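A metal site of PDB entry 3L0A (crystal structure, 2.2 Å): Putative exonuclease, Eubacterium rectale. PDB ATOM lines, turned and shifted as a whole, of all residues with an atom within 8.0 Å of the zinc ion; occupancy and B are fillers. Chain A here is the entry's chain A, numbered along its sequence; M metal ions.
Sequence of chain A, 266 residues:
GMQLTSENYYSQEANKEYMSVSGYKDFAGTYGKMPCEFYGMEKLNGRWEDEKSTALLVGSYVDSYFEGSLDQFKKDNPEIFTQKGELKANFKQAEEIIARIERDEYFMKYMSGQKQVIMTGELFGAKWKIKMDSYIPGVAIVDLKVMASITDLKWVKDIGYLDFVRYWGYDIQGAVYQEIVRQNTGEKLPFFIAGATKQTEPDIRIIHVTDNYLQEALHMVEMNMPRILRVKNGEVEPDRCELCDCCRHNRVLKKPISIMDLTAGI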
ATOM      1  N   ASP A  26      -9.188   9.187  20.852  1.00  0.00           N
ATOM      2  CA  ASP A  26      -8.815  10.613  20.945  1.00  0.00           C
ATOM      3  C   ASP A  26      -9.876  11.444  20.208  1.00  0.00           C
ATOM      4  O   ASP A  26     -10.477  12.380  20.762  1.00  0.00           O
ATOM      5  CB  ASP A  26      -7.431  10.911  20.352  1.00  0.00           C
ATOM      6  CG  ASP A  26      -6.254  10.308  21.168  1.00  0.00           C
ATOM      7  OD1 ASP A  26      -6.397  10.077  22.423  1.00  0.00           O
ATOM      8  OD2 ASP A  26      -5.179  10.067  20.527  1.00  0.00           O
ATOM      9  N   MET A  34     -15.062  12.766  26.991  1.00  0.00           N
ATOM     10  CA  MET A  34     -15.611  13.524  25.862  1.00  0.00           C
ATOM     11  C   MET A  34     -14.687  13.367  24.628  1.00  0.00           C
ATOM     12  O   MET A  34     -13.471  13.298  24.774  1.00  0.00           O
ATOM     13  CB  MET A  34     -15.784  15.038  26.230  1.00  0.00           C
ATOM     14  CG  MET A  34     -17.212  15.673  25.950  1.00  0.00           C
ATOM     15  SD  MET A  34     -18.709  14.541  26.661  1.00  0.00           S
ATOM     16  CE  MET A  34     -19.552  13.705  25.056  1.00  0.00           C
ATOM     17  N   PRO A  35     -15.250  13.310  23.417  1.00  0.00           N
ATOM     18  CA  PRO A  35     -14.360  13.405  22.264  1.00  0.00           C
ATOM     19  C   PRO A  35     -13.742  14.809  22.177  1.00  0.00           C
ATOM     20  O   PRO A  35     -14.330  15.784  22.682  1.00  0.00           O
ATOM     21  CB  PRO A  35     -15.287  13.158  21.067  1.00  0.00           C
ATOM     22  CG  PRO A  35     -16.640  13.549  21.536  1.00  0.00           C
ATOM     23  CD  PRO A  35     -16.679  13.281  23.018  1.00  0.00           C
ATOM     24  N   CYS A  36     -12.569  14.904  21.556  1.00  0.00           N
ATOM     25  CA  CYS A  36     -11.950  16.201  21.237  1.00  0.00           C
ATOM     26  C   CYS A  36     -11.010  16.037  20.051  1.00  0.00           C
ATOM     27  O   CYS A  36      -9.913  15.479  20.173  1.00  0.00           O
ATOM     28  CB  CYS A  36     -11.185  16.750  22.449  1.00  0.00           C
ATOM     29  SG  CYS A  36     -10.516  18.392  22.197  1.00  0.00           S
ATOM     30  N   GLU A  37     -11.450  16.550  18.898  1.00  0.00           N
ATOM     31  CA  GLU A  37     -10.716  16.392  17.631  1.00  0.00           C
ATOM     32  C   GLU A  37      -9.347  17.128  17.642  1.00  0.00           C
ATOM     33  O   GLU A  37      -8.324  16.590  17.208  1.00  0.00           O
ATOM     34  CB  GLU A  37     -11.598  16.880  16.473  1.00  0.00           C
ATOM     35  CG  GLU A  37     -12.924  16.124  16.403  1.00  0.00           C
ATOM     36  CD  GLU A  37     -13.782  16.412  15.182  1.00  0.00           C
ATOM     37  OE1 GLU A  37     -13.661  17.493  14.598  1.00  0.00           O
ATOM     38  OE2 GLU A  37     -14.594  15.534  14.783  1.00  0.00           O
ATOM     39  N   PHE A  38      -9.372  18.354  18.159  1.00  0.00           N
ATOM     40  CA  PHE A  38      -8.210  19.185  18.352  1.00  0.00           C
ATOM     41  C   PHE A  38      -7.133  18.456  19.145  1.00  0.00           C
ATOM     42  O   PHE A  38      -6.013  18.333  18.688  1.00  0.00           O
ATOM     43  CB  PHE A  38      -8.673  20.444  19.088  1.00  0.00           C
ATOM     44  CG  PHE A  38      -7.580  21.425  19.392  1.00  0.00           C
ATOM     45  CD1 PHE A  38      -6.909  22.082  18.368  1.00  0.00           C
ATOM     46  CD2 PHE A  38      -7.236  21.713  20.704  1.00  0.00           C
ATOM     47  CE1 PHE A  38      -5.904  22.987  18.664  1.00  0.00           C
ATOM     48  CE2 PHE A  38      -6.228  22.608  20.990  1.00  0.00           C
ATOM     49  CZ  PHE A  38      -5.562  23.246  19.987  1.00  0.00           C
ATOM     50  N   TYR A  39      -7.497  17.940  20.326  1.00  0.00           N
ATOM     51  CA  TYR A  39      -6.582  17.153  21.139  1.00  0.00           C
ATOM     52  C   TYR A  39      -5.927  16.042  20.341  1.00  0.00           C
ATOM     53  O   TYR A  39      -4.717  15.801  20.445  1.00  0.00           O
ATOM     54  CB  TYR A  39      -7.325  16.556  22.327  1.00  0.00           C
ATOM     55  CG  TYR A  39      -6.615  15.476  23.114  1.00  0.00           C
ATOM     56  CD1 TYR A  39      -5.538  15.770  23.928  1.00  0.00           C
ATOM     57  CD2 TYR A  39      -7.049  14.158  23.052  1.00  0.00           C
ATOM     58  CE1 TYR A  39      -4.885  14.756  24.684  1.00  0.00           C
ATOM     59  CE2 TYR A  39      -6.427  13.133  23.808  1.00  0.00           C
ATOM     60  CZ  TYR A  39      -5.348  13.446  24.612  1.00  0.00           C
ATOM     61  OH  TYR A  39      -4.724  12.449  25.326  1.00  0.00           O
ATOM     62  N   GLY A  40      -6.731  15.393  19.508  1.00  0.00           N
ATOM     63  CA  GLY A  40      -6.246  14.332  18.672  1.00  0.00           C
ATOM     64  C   GLY A  40      -5.251  14.756  17.615  1.00  0.00           C
ATOM     65  O   GLY A  40      -4.346  13.983  17.259  1.00  0.00           O
ATOM     66  N   ASP A 239     -12.843  20.326  15.718  1.00  0.00           N
ATOM     67  CA  ASP A 239     -13.516  20.994  16.833  1.00  0.00           C
ATOM     68  C   ASP A 239     -12.729  20.826  18.144  1.00  0.00           C
ATOM     69  O   ASP A 239     -12.022  19.858  18.336  1.00  0.00           O
ATOM     70  CB  ASP A 239     -14.927  20.412  17.038  1.00  0.00           C
ATOM     71  CG  ASP A 239     -15.853  20.656  15.837  1.00  0.00           C
ATOM     72  OD1 ASP A 239     -15.725  21.694  15.118  1.00  0.00           O
ATOM     73  OD2 ASP A 239     -16.727  19.781  15.617  1.00  0.00           O
ATOM     74  N   ARG A 240     -12.911  21.774  19.045  1.00  0.00           N
ATOM     75  CA  ARG A 240     -12.321  21.736  20.382  1.00  0.00           C
ATOM     76  C   ARG A 240     -13.407  21.477  21.395  1.00  0.00           C
ATOM     77  O   ARG A 240     -14.408  22.174  21.401  1.00  0.00           O
ATOM     78  CB  ARG A 240     -11.699  23.092  20.689  1.00  0.00           C
ATOM     79  CG  ARG A 240     -10.612  23.504  19.737  1.00  0.00           C
ATOM     80  CD  ARG A 240      -9.861  24.713  20.281  1.00  0.00           C
ATOM     81  NE  ARG A 240      -8.800  25.174  19.363  1.00  0.00           N
ATOM     82  CZ  ARG A 240      -7.894  26.095  19.666  1.00  0.00           C
ATOM     83  NH1 ARG A 240      -7.894  26.691  20.845  1.00  0.00           N
ATOM     84  NH2 ARG A 240      -6.983  26.458  18.772  1.00  0.00           N
ATOM     85  N   CYS A 241     -13.198  20.503  22.293  1.00  0.00           N
ATOM     86  CA  CYS A 241     -14.181  20.209  23.321  1.00  0.00           C
ATOM     87  C   CYS A 241     -14.191  21.360  24.300  1.00  0.00           C
ATOM     88  O   CYS A 241     -15.180  21.587  24.971  1.00  0.00           O
ATOM     89  CB  CYS A 241     -13.883  18.905  24.052  1.00  0.00           C
ATOM     90  SG  CYS A 241     -12.412  18.907  25.133  1.00  0.00           S
ATOM     91  N   GLU A 242     -13.078  22.064  24.381  1.00  0.00           N
ATOM     92  CA  GLU A 242     -12.916  23.154  25.335  1.00  0.00           C
ATOM     93  C   GLU A 242     -13.042  22.680  26.800  1.00  0.00           C
ATOM     94  O   GLU A 242     -13.223  23.498  27.691  1.00  0.00           O
ATOM     95  CB  GLU A 242     -13.877  24.325  25.043  1.00  0.00           C
ATOM     96  CG  GLU A 242     -13.719  24.994  23.662  1.00  0.00           C
ATOM     97  CD  GLU A 242     -12.456  25.891  23.550  1.00  0.00           C
ATOM     98  OE1 GLU A 242     -11.619  25.985  24.484  1.00  0.00           O
ATOM     99  OE2 GLU A 242     -12.292  26.520  22.499  1.00  0.00           O
ATOM    100  N   LEU A 243     -12.904  21.392  27.042  1.00  0.00           N
ATOM    101  CA  LEU A 243     -12.983  20.846  28.385  1.00  0.00           C
ATOM    102  C   LEU A 243     -11.766  19.993  28.795  1.00  0.00           C
ATOM    103  O   LEU A 243     -11.785  19.383  29.854  1.00  0.00           O
ATOM    104  CB  LEU A 243     -14.286  20.018  28.536  1.00  0.00           C
ATOM    105  CG  LEU A 243     -15.599  20.825  28.443  1.00  0.00           C
ATOM    106  CD1 LEU A 243     -16.853  19.887  28.506  1.00  0.00           C
ATOM    107  CD2 LEU A 243     -15.685  21.886  29.566  1.00  0.00           C
ATOM    108  N   CYS A 244     -10.715  19.936  27.974  1.00  0.00           N
ATOM    109  CA  CYS A 244      -9.535  19.147  28.265  1.00  0.00           C
ATOM    110  C   CYS A 244      -8.357  20.100  28.482  1.00  0.00           C
ATOM    111  O   CYS A 244      -8.440  21.310  28.218  1.00  0.00           O
ATOM    112  CB  CYS A 244      -9.259  18.156  27.101  1.00  0.00           C
ATOM    113  SG  CYS A 244      -8.782  18.998  25.564  1.00  0.00           S
ATOM    114  N   ASP A 245      -7.253  19.564  28.976  1.00  0.00           N
ATOM    115  CA  ASP A 245      -6.094  20.369  29.337  1.00  0.00           C
ATOM    116  C   ASP A 245      -5.467  21.007  28.076  1.00  0.00           C
ATOM    117  O   ASP A 245      -5.035  22.194  28.107  1.00  0.00           O
ATOM    118  CB  ASP A 245      -5.068  19.527  30.114  1.00  0.00           C
ATOM    119  CG  ASP A 245      -5.436  19.301  31.619  1.00  0.00           C
ATOM    120  OD1 ASP A 245      -6.107  20.155  32.267  1.00  0.00           O
ATOM    121  OD2 ASP A 245      -4.980  18.280  32.180  1.00  0.00           O
ATOM    122  N   CYS A 246      -5.430  20.255  26.976  1.00  0.00           N
ATOM    123  CA  CYS A 246      -4.908  20.756  25.680  1.00  0.00           C
ATOM    124  C   CYS A 246      -5.708  21.961  25.220  1.00  0.00           C
ATOM    125  O   CYS A 246      -5.141  23.005  24.918  1.00  0.00           O
ATOM    126  CB  CYS A 246      -4.966  19.658  24.581  1.00  0.00           C
ATOM    127  SG  CYS A 246      -4.371  20.153  22.951  1.00  0.00           S
ATOM    128  N   CYS A 247      -7.024  21.819  25.221  1.00  0.00           N
ATOM    129  CA  CYS A 247      -7.912  22.934  24.912  1.00  0.00           C
ATOM    130  C   CYS A 247      -7.620  24.157  25.772  1.00  0.00           C
ATOM    131  O   CYS A 247      -7.572  25.277  25.269  1.00  0.00           O
ATOM    132  CB  CYS A 247      -9.372  22.507  25.046  1.00  0.00           C
ATOM    133  SG  CYS A 247     -10.082  21.842  23.516  1.00  0.00           S
ATOM    134  N   ARG A 248      -7.404  23.947  27.056  1.00  0.00           N
ATOM    135  CA  ARG A 248      -7.224  25.046  27.985  1.00  0.00           C
ATOM    136  C   ARG A 248      -5.872  25.726  27.811  1.00  0.00           C
ATOM    137  O   ARG A 248      -5.779  26.956  27.893  1.00  0.00           O
ATOM    138  CB  ARG A 248      -7.401  24.599  29.442  1.00  0.00           C
ATOM    139  CG  ARG A 248      -8.818  24.081  29.772  1.00  0.00           C
ATOM    140  CD  ARG A 248      -9.093  24.020  31.254  1.00  0.00           C
ATOM    141  NE  ARG A 248      -8.664  22.737  31.787  1.00  0.00           N
ATOM    142  CZ  ARG A 248      -9.378  21.624  31.732  1.00  0.00           C
ATOM    143  NH1 ARG A 248     -10.577  21.592  31.190  1.00  0.00           N
ATOM    144  NH2 ARG A 248      -8.873  20.524  32.225  1.00  0.00           N
ATOM    145  N   ARG A 251      -6.151  28.021  24.630  1.00  0.00           N
ATOM    146  CA  ARG A 251      -7.208  29.011  24.497  1.00  0.00           C
ATOM    147  C   ARG A 251      -6.629  30.395  24.492  1.00  0.00           C
ATOM    148  O   ARG A 251      -5.724  30.668  25.258  1.00  0.00           O
ATOM    149  CB  ARG A 251      -8.227  28.879  25.627  1.00  0.00           C
ATOM    150  CG  ARG A 251      -9.396  29.843  25.487  1.00  0.00           C
ATOM    151  CD  ARG A 251     -10.490  29.563  26.497  1.00  0.00           C
ATOM    152  NE  ARG A 251     -10.761  28.128  26.599  1.00  0.00           N
ATOM    153  CZ  ARG A 251     -11.247  27.533  27.686  1.00  0.00           C
ATOM    154  NH1 ARG A 251     -11.519  28.242  28.770  1.00  0.00           N
ATOM    155  NH2 ARG A 251     -11.441  26.220  27.697  1.00  0.00           N
HETATM  156 ZN    ZN M   1     -10.406  19.446  24.075  1.00  0.00          ZN
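The side-chain sulfur of Cys 36 lies close to the backbone NH of Tyr 39 (3.6 Å).
The backbone NH of Cys 36 is in hydrogen-bond range of the backbone carbonyl oxygen of Asp 26, at 3.4 Å.
The side-chain sulfur (SG) of Cys 241 sits close to the backbone NH (N) of Leu 243 (3.2 Å).
SG of Cys 247 lies close to N of Glu 242, 3.1 Å away.
NE of Arg 251 lies within salt-bridge range of OE1 of Glu 242 (3.1 Å).
Glu 242 touches the zinc ion.
Within 4 Å of the zinc ion: Cys 36, Cys 241, Glu 242, Cys 244 and Cys 247.
The zinc ion is bound by SG of Cys 36 (2.2 Å).
The zinc ion is bound by SG of Cys 244 (2.2 Å).
The zinc ion is bound by SG of Cys 241 (2.3 Å).
The zinc ion is bound by SG of Cys 247 (2.5 Å).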
